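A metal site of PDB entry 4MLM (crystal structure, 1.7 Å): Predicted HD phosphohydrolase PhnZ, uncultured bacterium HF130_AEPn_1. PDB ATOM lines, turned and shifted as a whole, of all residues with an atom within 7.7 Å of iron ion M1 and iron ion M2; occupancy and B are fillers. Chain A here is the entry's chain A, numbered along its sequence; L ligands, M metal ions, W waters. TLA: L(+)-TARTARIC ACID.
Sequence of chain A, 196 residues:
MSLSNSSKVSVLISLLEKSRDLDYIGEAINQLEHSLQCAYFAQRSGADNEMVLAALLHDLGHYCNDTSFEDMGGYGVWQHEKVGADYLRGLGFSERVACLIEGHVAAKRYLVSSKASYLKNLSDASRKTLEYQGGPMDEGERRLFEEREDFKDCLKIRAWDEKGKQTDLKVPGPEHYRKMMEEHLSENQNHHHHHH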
ATOM      1  N   TYR A  24       3.512   7.824  16.598  1.00  0.00           N
ATOM      2  CA  TYR A  24       2.296   8.566  16.301  1.00  0.00           C
ATOM      3  C   TYR A  24       2.651   9.786  15.469  1.00  0.00           C
ATOM      4  O   TYR A  24       2.232   9.918  14.316  1.00  0.00           O
ATOM      5  CB  TYR A  24       1.535   8.960  17.569  1.00  0.00           C
ATOM      6  CG  TYR A  24       0.092   9.304  17.284  1.00  0.00           C
ATOM      7  CD1 TYR A  24      -0.870   8.310  17.210  1.00  0.00           C
ATOM      8  CD2 TYR A  24      -0.306  10.614  17.051  1.00  0.00           C
ATOM      9  CE1 TYR A  24      -2.209   8.606  16.927  1.00  0.00           C
ATOM     10  CE2 TYR A  24      -1.626  10.924  16.767  1.00  0.00           C
ATOM     11  CZ  TYR A  24      -2.579   9.933  16.719  1.00  0.00           C
ATOM     12  OH  TYR A  24      -3.899  10.244  16.435  1.00  0.00           O
ATOM     13  N   GLN A  31       2.391   6.666  20.437  1.00  0.00           N
ATOM     14  CA  GLN A  31       0.941   6.632  20.600  1.00  0.00           C
ATOM     15  C   GLN A  31       0.508   6.791  22.044  1.00  0.00           C
ATOM     16  O   GLN A  31      -0.552   7.372  22.323  1.00  0.00           O
ATOM     17  CB  GLN A  31       0.363   5.344  20.014  1.00  0.00           C
ATOM     18  CG  GLN A  31      -1.152   5.342  19.954  1.00  0.00           C
ATOM     19  CD  GLN A  31      -1.688   4.097  19.305  1.00  0.00           C
ATOM     20  OE1 GLN A  31      -1.497   3.898  18.088  1.00  0.00           O
ATOM     21  NE2 GLN A  31      -2.321   3.228  20.088  1.00  0.00           N
ATOM     22  N   HIS A  34       0.730  10.409  22.966  1.00  0.00           N
ATOM     23  CA  HIS A  34      -0.387  11.081  22.300  1.00  0.00           C
ATOM     24  C   HIS A  34      -1.690  10.897  23.070  1.00  0.00           C
ATOM     25  O   HIS A  34      -2.421  11.861  23.312  1.00  0.00           O
ATOM     26  CB  HIS A  34      -0.548  10.536  20.869  1.00  0.00           C
ATOM     27  CG  HIS A  34      -1.875  10.850  20.242  1.00  0.00           C
ATOM     28  ND1 HIS A  34      -2.247  12.124  19.869  1.00  0.00           N
ATOM     29  CD2 HIS A  34      -2.906  10.040  19.875  1.00  0.00           C
ATOM     30  CE1 HIS A  34      -3.454  12.095  19.342  1.00  0.00           C
ATOM     31  NE2 HIS A  34      -3.873  10.845  19.329  1.00  0.00           N
ATOM     32  N   SER A  35      -1.961   9.663  23.449  1.00  0.00           N
ATOM     33  CA  SER A  35      -3.204   9.343  24.149  1.00  0.00           C
ATOM     34  C   SER A  35      -3.287  10.043  25.492  1.00  0.00           C
ATOM     35  O   SER A  35      -4.351  10.514  25.891  1.00  0.00           O
ATOM     36  CB  SER A  35      -3.327   7.826  24.348  1.00  0.00           C
ATOM     37  OG  SER A  35      -3.277   7.175  23.093  1.00  0.00           O
ATOM     38  N   CYS A  38      -4.058  13.716  25.056  1.00  0.00           N
ATOM     39  CA  CYS A  38      -5.481  13.905  24.769  1.00  0.00           C
ATOM     40  C   CYS A  38      -6.343  13.802  26.021  1.00  0.00           C
ATOM     41  O   CYS A  38      -7.243  14.606  26.219  1.00  0.00           O
ATOM     42  CB  CYS A  38      -5.968  12.892  23.737  1.00  0.00           C
ATOM     43  SG  CYS A  38      -5.261  13.167  22.118  1.00  0.00           S
ATOM     44  N   ALA A  55     -11.052  10.197  25.316  1.00  0.00           N
ATOM     45  CA  ALA A  55      -9.806  10.804  24.835  1.00  0.00           C
ATOM     46  C   ALA A  55      -8.607   9.893  25.106  1.00  0.00           C
ATOM     47  O   ALA A  55      -7.737   9.715  24.247  1.00  0.00           O
ATOM     48  CB  ALA A  55      -9.603  12.171  25.474  1.00  0.00           C
ATOM     49  N   HIS A  58      -8.997   6.552  22.704  1.00  0.00           N
ATOM     50  CA  HIS A  58      -9.534   6.632  21.342  1.00  0.00           C
ATOM     51  C   HIS A  58      -8.692   5.897  20.291  1.00  0.00           C
ATOM     52  O   HIS A  58      -9.223   5.492  19.250  1.00  0.00           O
ATOM     53  CB  HIS A  58      -9.792   8.083  20.901  1.00  0.00           C
ATOM     54  CG  HIS A  58      -8.549   8.843  20.529  1.00  0.00           C
ATOM     55  ND1 HIS A  58      -7.709   9.389  21.473  1.00  0.00           N
ATOM     56  CD2 HIS A  58      -8.042   9.175  19.322  1.00  0.00           C
ATOM     57  CE1 HIS A  58      -6.711  10.007  20.870  1.00  0.00           C
ATOM     58  NE2 HIS A  58      -6.882   9.896  19.560  1.00  0.00           N
ATOM     59  N   ASP A  59      -7.406   5.726  20.554  1.00  0.00           N
ATOM     60  CA  ASP A  59      -6.529   5.117  19.552  1.00  0.00           C
ATOM     61  C   ASP A  59      -6.058   3.719  19.937  1.00  0.00           C
ATOM     62  O   ASP A  59      -5.188   3.146  19.278  1.00  0.00           O
ATOM     63  CB  ASP A  59      -5.317   6.026  19.284  1.00  0.00           C
ATOM     64  CG  ASP A  59      -5.646   7.127  18.281  1.00  0.00           C
ATOM     65  OD1 ASP A  59      -6.629   6.963  17.509  1.00  0.00           O
ATOM     66  OD2 ASP A  59      -4.906   8.139  18.277  1.00  0.00           O
ATOM     67  N   LEU A  60      -6.645   3.151  20.976  1.00  0.00           N
ATOM     68  CA  LEU A  60      -6.207   1.843  21.451  1.00  0.00           C
ATOM     69  C   LEU A  60      -6.300   0.793  20.345  1.00  0.00           C
ATOM     70  O   LEU A  60      -5.529  -0.178  20.316  1.00  0.00           O
ATOM     71  CB  LEU A  60      -7.043   1.424  22.658  1.00  0.00           C
ATOM     72  CG  LEU A  60      -6.377   0.387  23.564  1.00  0.00           C
ATOM     73  CD1 LEU A  60      -5.072   0.920  24.123  1.00  0.00           C
ATOM     74  CD2 LEU A  60      -7.319  -0.031  24.679  1.00  0.00           C
ATOM     75  N   HIS A  62      -5.457   0.674  17.215  1.00  0.00           N
ATOM     76  CA  HIS A  62      -4.443   0.547  16.175  1.00  0.00           C
ATOM     77  C   HIS A  62      -3.667  -0.765  16.344  1.00  0.00           C
ATOM     78  O   HIS A  62      -3.280  -1.123  17.445  1.00  0.00           O
ATOM     79  CB  HIS A  62      -3.433   1.701  16.236  1.00  0.00           C
ATOM     80  CG  HIS A  62      -3.912   2.987  15.612  1.00  0.00           C
ATOM     81  ND1 HIS A  62      -4.333   3.060  14.302  1.00  0.00           N
ATOM     82  CD2 HIS A  62      -3.974   4.237  16.106  1.00  0.00           C
ATOM     83  CE1 HIS A  62      -4.684   4.303  14.030  1.00  0.00           C
ATOM     84  NE2 HIS A  62      -4.459   5.050  15.108  1.00  0.00           N
ATOM     85  N   HIS A  80      -9.249   1.214  13.334  1.00  0.00           N
ATOM     86  CA  HIS A  80      -8.920   1.346  14.754  1.00  0.00           C
ATOM     87  C   HIS A  80     -10.042   1.910  15.588  1.00  0.00           C
ATOM     88  O   HIS A  80     -10.214   1.510  16.745  1.00  0.00           O
ATOM     89  CB  HIS A  80      -7.619   2.131  14.997  1.00  0.00           C
ATOM     90  CG  HIS A  80      -7.751   3.625  14.809  1.00  0.00           C
ATOM     91  ND1 HIS A  80      -8.028   4.197  13.592  1.00  0.00           N
ATOM     92  CD2 HIS A  80      -7.593   4.651  15.679  1.00  0.00           C
ATOM     93  CE1 HIS A  80      -8.059   5.508  13.724  1.00  0.00           C
ATOM     94  NE2 HIS A  80      -7.794   5.816  14.978  1.00  0.00           N
ATOM     95  N   GLU A  81     -10.810   2.850  15.027  1.00  0.00           N
ATOM     96  CA  GLU A  81     -11.913   3.446  15.776  1.00  0.00           C
ATOM     97  C   GLU A  81     -12.990   2.409  16.105  1.00  0.00           C
ATOM     98  O   GLU A  81     -13.625   2.469  17.171  1.00  0.00           O
ATOM     99  CB  GLU A  81     -12.499   4.666  15.053  1.00  0.00           C
ATOM    100  CG  GLU A  81     -13.407   4.372  13.861  1.00  0.00           C
ATOM    101  CD  GLU A  81     -12.651   4.064  12.576  1.00  0.00           C
ATOM    102  OE1 GLU A  81     -11.415   3.845  12.613  1.00  0.00           O
ATOM    103  OE2 GLU A  81     -13.307   4.041  11.506  1.00  0.00           O
ATOM    104  N   ILE A 101     -15.418   7.404  20.675  1.00  0.00           N
ATOM    105  CA  ILE A 101     -14.227   6.815  20.069  1.00  0.00           C
ATOM    106  C   ILE A 101     -14.501   6.428  18.633  1.00  0.00           C
ATOM    107  O   ILE A 101     -13.721   6.748  17.727  1.00  0.00           O
ATOM    108  CB  ILE A 101     -13.750   5.589  20.874  1.00  0.00           C
ATOM    109  CG1 ILE A 101     -13.224   6.046  22.233  1.00  0.00           C
ATOM    110  CG2 ILE A 101     -12.661   4.808  20.100  1.00  0.00           C
ATOM    111  CD1 ILE A 101     -12.761   4.927  23.164  1.00  0.00           C
ATOM    112  N   HIS A 104     -14.516   9.359  15.946  1.00  0.00           N
ATOM    113  CA  HIS A 104     -13.441  10.359  15.773  1.00  0.00           C
ATOM    114  C   HIS A 104     -12.877  10.422  14.363  1.00  0.00           C
ATOM    115  O   HIS A 104     -12.273  11.432  13.977  1.00  0.00           O
ATOM    116  CB  HIS A 104     -12.337  10.272  16.858  1.00  0.00           C
ATOM    117  CG  HIS A 104     -11.239   9.288  16.587  1.00  0.00           C
ATOM    118  ND1 HIS A 104     -11.341   7.939  16.871  1.00  0.00           N
ATOM    119  CD2 HIS A 104      -9.965   9.474  16.149  1.00  0.00           C
ATOM    120  CE1 HIS A 104     -10.202   7.336  16.584  1.00  0.00           C
ATOM    121  NE2 HIS A 104      -9.343   8.241  16.142  1.00  0.00           N
ATOM    122  N   VAL A 105     -13.113   9.395  13.557  1.00  0.00           N
ATOM    123  CA  VAL A 105     -12.780   9.485  12.145  1.00  0.00           C
ATOM    124  C   VAL A 105     -13.804  10.356  11.423  1.00  0.00           C
ATOM    125  O   VAL A 105     -13.439  11.247  10.643  1.00  0.00           O
ATOM    126  CB  VAL A 105     -12.655   8.114  11.472  1.00  0.00           C
ATOM    127  CG1 VAL A 105     -12.646   8.263   9.950  1.00  0.00           C
ATOM    128  CG2 VAL A 105     -11.377   7.431  11.966  1.00  0.00           C
ATOM    129  N   SER A 126      -3.099  11.054   9.077  1.00  0.00           N
ATOM    130  CA  SER A 126      -4.499  11.467   9.077  1.00  0.00           C
ATOM    131  C   SER A 126      -4.923  12.029   7.723  1.00  0.00           C
ATOM    132  O   SER A 126      -6.066  11.858   7.290  1.00  0.00           O
ATOM    133  CB  SER A 126      -4.774  12.483  10.189  1.00  0.00           C
ATOM    134  OG  SER A 126      -4.651  11.862  11.457  1.00  0.00           O
ATOM    135  N   GLN A 133     -11.438   7.012   3.584  1.00  0.00           N
ATOM    136  CA  GLN A 133     -12.544   7.100   4.532  1.00  0.00           C
ATOM    137  C   GLN A 133     -13.714   7.845   3.920  1.00  0.00           C
ATOM    138  O   GLN A 133     -14.675   8.194   4.607  1.00  0.00           O
ATOM    139  CB  GLN A 133     -12.063   7.795   5.802  1.00  0.00           C
ATOM    140  CG  GLN A 133     -11.014   7.001   6.551  1.00  0.00           C
ATOM    141  CD  GLN A 133     -10.218   7.826   7.549  1.00  0.00           C
ATOM    142  OE1 GLN A 133     -10.154   9.059   7.449  1.00  0.00           O
ATOM    143  NE2 GLN A 133      -9.591   7.162   8.512  1.00  0.00           N
ATOM    144  N   ILE A 157     -13.325  15.865  20.899  1.00  0.00           N
ATOM    145  CA  ILE A 157     -12.395  14.740  20.903  1.00  0.00           C
ATOM    146  C   ILE A 157     -11.394  14.855  19.755  1.00  0.00           C
ATOM    147  O   ILE A 157     -10.199  14.617  19.943  1.00  0.00           O
ATOM    148  CB  ILE A 157     -13.147  13.377  20.790  1.00  0.00           C
ATOM    149  CG1 ILE A 157     -13.947  13.098  22.066  1.00  0.00           C
ATOM    150  CG2 ILE A 157     -12.164  12.234  20.502  1.00  0.00           C
ATOM    151  CD1 ILE A 157     -13.105  12.856  23.279  1.00  0.00           C
ATOM    152  N   ARG A 158     -11.868  15.222  18.568  1.00  0.00           N
ATOM    153  CA  ARG A 158     -10.960  15.270  17.429  1.00  0.00           C
ATOM    154  C   ARG A 158     -10.069  16.520  17.458  1.00  0.00           C
ATOM    155  O   ARG A 158      -8.902  16.470  17.062  1.00  0.00           O
ATOM    156  CB  ARG A 158     -11.717  15.148  16.097  1.00  0.00           C
ATOM    157  CG  ARG A 158     -10.780  15.073  14.880  1.00  0.00           C
ATOM    158  CD  ARG A 158     -10.245  13.660  14.692  1.00  0.00           C
ATOM    159  NE  ARG A 158      -8.947  13.645  14.009  1.00  0.00           N
ATOM    160  CZ  ARG A 158      -8.421  12.563  13.459  1.00  0.00           C
ATOM    161  NH1 ARG A 158      -9.119  11.434  13.464  1.00  0.00           N
ATOM    162  NH2 ARG A 158      -7.227  12.603  12.886  1.00  0.00           N
ATOM    163  N   TRP A 160      -8.903  17.804  20.196  1.00  0.00           N
ATOM    164  CA  TRP A 160      -7.858  17.435  21.156  1.00  0.00           C
ATOM    165  C   TRP A 160      -6.877  16.464  20.502  1.00  0.00           C
ATOM    166  O   TRP A 160      -5.679  16.554  20.686  1.00  0.00           O
ATOM    167  CB  TRP A 160      -8.464  16.810  22.418  1.00  0.00           C
ATOM    168  CG  TRP A 160      -9.298  17.796  23.201  1.00  0.00           C
ATOM    169  CD1 TRP A 160      -9.104  19.147  23.306  1.00  0.00           C
ATOM    170  CD2 TRP A 160     -10.460  17.495  23.992  1.00  0.00           C
ATOM    171  NE1 TRP A 160     -10.078  19.697  24.108  1.00  0.00           N
ATOM    172  CE2 TRP A 160     -10.920  18.699  24.542  1.00  0.00           C
ATOM    173  CE3 TRP A 160     -11.156  16.317  24.287  1.00  0.00           C
ATOM    174  CZ2 TRP A 160     -12.043  18.770  25.370  1.00  0.00           C
ATOM    175  CZ3 TRP A 160     -12.261  16.384  25.103  1.00  0.00           C
ATOM    176  CH2 TRP A 160     -12.706  17.601  25.638  1.00  0.00           C
ATOM    177  N   ASP A 161      -7.422  15.542  19.725  1.00  0.00           N
ATOM    178  CA  ASP A 161      -6.621  14.593  18.963  1.00  0.00           C
ATOM    179  C   ASP A 161      -5.535  15.285  18.141  1.00  0.00           C
ATOM    180  O   ASP A 161      -4.349  14.940  18.249  1.00  0.00           O
ATOM    181  CB  ASP A 161      -7.590  13.813  18.061  1.00  0.00           C
ATOM    182  CG  ASP A 161      -6.974  12.620  17.413  1.00  0.00           C
ATOM    183  OD1 ASP A 161      -5.843  12.232  17.762  1.00  0.00           O
ATOM    184  OD2 ASP A 161      -7.660  12.050  16.526  1.00  0.00           O
ATOM    185  N   GLU A 162      -5.919  16.273  17.335  1.00  0.00           N
ATOM    186  CA  GLU A 162      -4.927  16.967  16.507  1.00  0.00           C
ATOM    187  C   GLU A 162      -3.931  17.741  17.348  1.00  0.00           C
ATOM    188  O   GLU A 162      -2.791  17.977  16.919  1.00  0.00           O
ATOM    189  CB  GLU A 162      -5.597  17.895  15.496  1.00  0.00           C
ATOM    190  CG  GLU A 162      -5.634  17.335  14.078  1.00  0.00           C
ATOM    191  CD  GLU A 162      -6.433  16.049  13.985  1.00  0.00           C
ATOM    192  OE1 GLU A 162      -7.670  16.103  14.104  1.00  0.00           O
ATOM    193  OE2 GLU A 162      -5.815  14.960  13.796  1.00  0.00           O
ATOM    194  N   GLY A 164      -2.764  16.692  20.228  1.00  0.00           N
ATOM    195  CA  GLY A 164      -1.967  15.774  21.031  1.00  0.00           C
ATOM    196  C   GLY A 164      -0.618  15.409  20.427  1.00  0.00           C
ATOM    197  O   GLY A 164      -0.315  14.228  20.211  1.00  0.00           O
HETATM  198  O1  TLA L   1      -3.676   8.267  13.660  1.00  0.00           O
HETATM  199  O11 TLA L   1      -5.201   7.538  15.074  1.00  0.00           O
HETATM  200  C1  TLA L   1      -4.878   8.199  14.036  1.00  0.00           C
HETATM  201  C2  TLA L   1      -5.937   8.889  13.244  1.00  0.00           C
HETATM  202  O2  TLA L   1      -7.174   8.650  13.841  1.00  0.00           O
HETATM  203  C3  TLA L   1      -5.876   8.364  11.856  1.00  0.00           C
HETATM  204  O3  TLA L   1      -5.917   6.987  11.854  1.00  0.00           O
HETATM  205  C4  TLA L   1      -7.048   8.888  11.114  1.00  0.00           C
HETATM  206  O4  TLA L   1      -7.259  10.129  11.067  1.00  0.00           O
HETATM  207  O41 TLA L   1      -7.815   8.081  10.546  1.00  0.00           O
HETATM  208 FE    FE M   1      -5.374  10.144  18.017  1.00  0.00          FE
HETATM  209 FE    FE M   2      -7.224   7.829  15.716  1.00  0.00          FE
HETATM  210  O   HOH W   1      -6.658   9.837  16.403  1.00  0.00           O
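A ring nitrogen (ND1) of His 58 is in hydrogen-bond range of the backbone carbonyl oxygen (O) of Ala 55 (2.8 Å). SG of Cys 38 is in hydrogen-bond range of O of His 34. A ring nitrogen (ND1) of His 104 is in hydrogen-bond range of the backbone carbonyl oxygen of Ile 101 (2.8 Å). The backbone carbonyl oxygen (O) of Gly 164 sits at hydrogen-bond distance from a ring nitrogen (ND1) of His 34 (2.9 Å). The backbone carbonyl oxygen of His 104 sits close to the guanidinium group of Arg 158, at 3.2 Å. The backbone carbonyl oxygen (O) of Asp 59 sits at hydrogen-bond distance from the side-chain amide nitrogen (NE2) of Gln 31 (3.0 Å). The guanidinium group (NE) of Arg 158 lies within salt-bridge range of the side-chain carboxylate (OD2) of Asp 161 (3.2 Å). NE2 of His 80 lies close to NE2 of His 62 (3.4 Å).
Five residues have an atom within 4 Å of iron ion M1: Tyr 24, His 34, His 58, Asp 59 and Asp 161.
Merely in contact with iron ion M2: His 62 (3.97 Å). Of the 23 residues printed, 5 come within 4 Å of iron ion M2. Along chain A the residues within 4 Å of iron ion M2 span positions 58 to 104.
Iron ion M1 is bound by the side-chain carboxylate of Asp 59 (2.1 Å), water W1 (2.1 Å), a ring nitrogen (NE2) of His 34 (2.1 Å), the side-chain carboxylate of Asp 161 (2.2 Å), the side-chain hydroxyl of Tyr 24 (2.2 Å) and a ring nitrogen (NE2) of His 58 (2.2 Å). Iron ion M1 has six donor atoms within binding distance.
Iron ion M2 is bound by O2 of the ligand (2.0 Å), OD1 of Asp 59 (2.1 Å), O11 of the ligand (2.1 Å), water W1 (2.2 Å), NE2 of His 104 (2.2 Å) and NE2 of His 80 (2.2 Å). Iron ion M2 has six donor atoms within binding distance.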
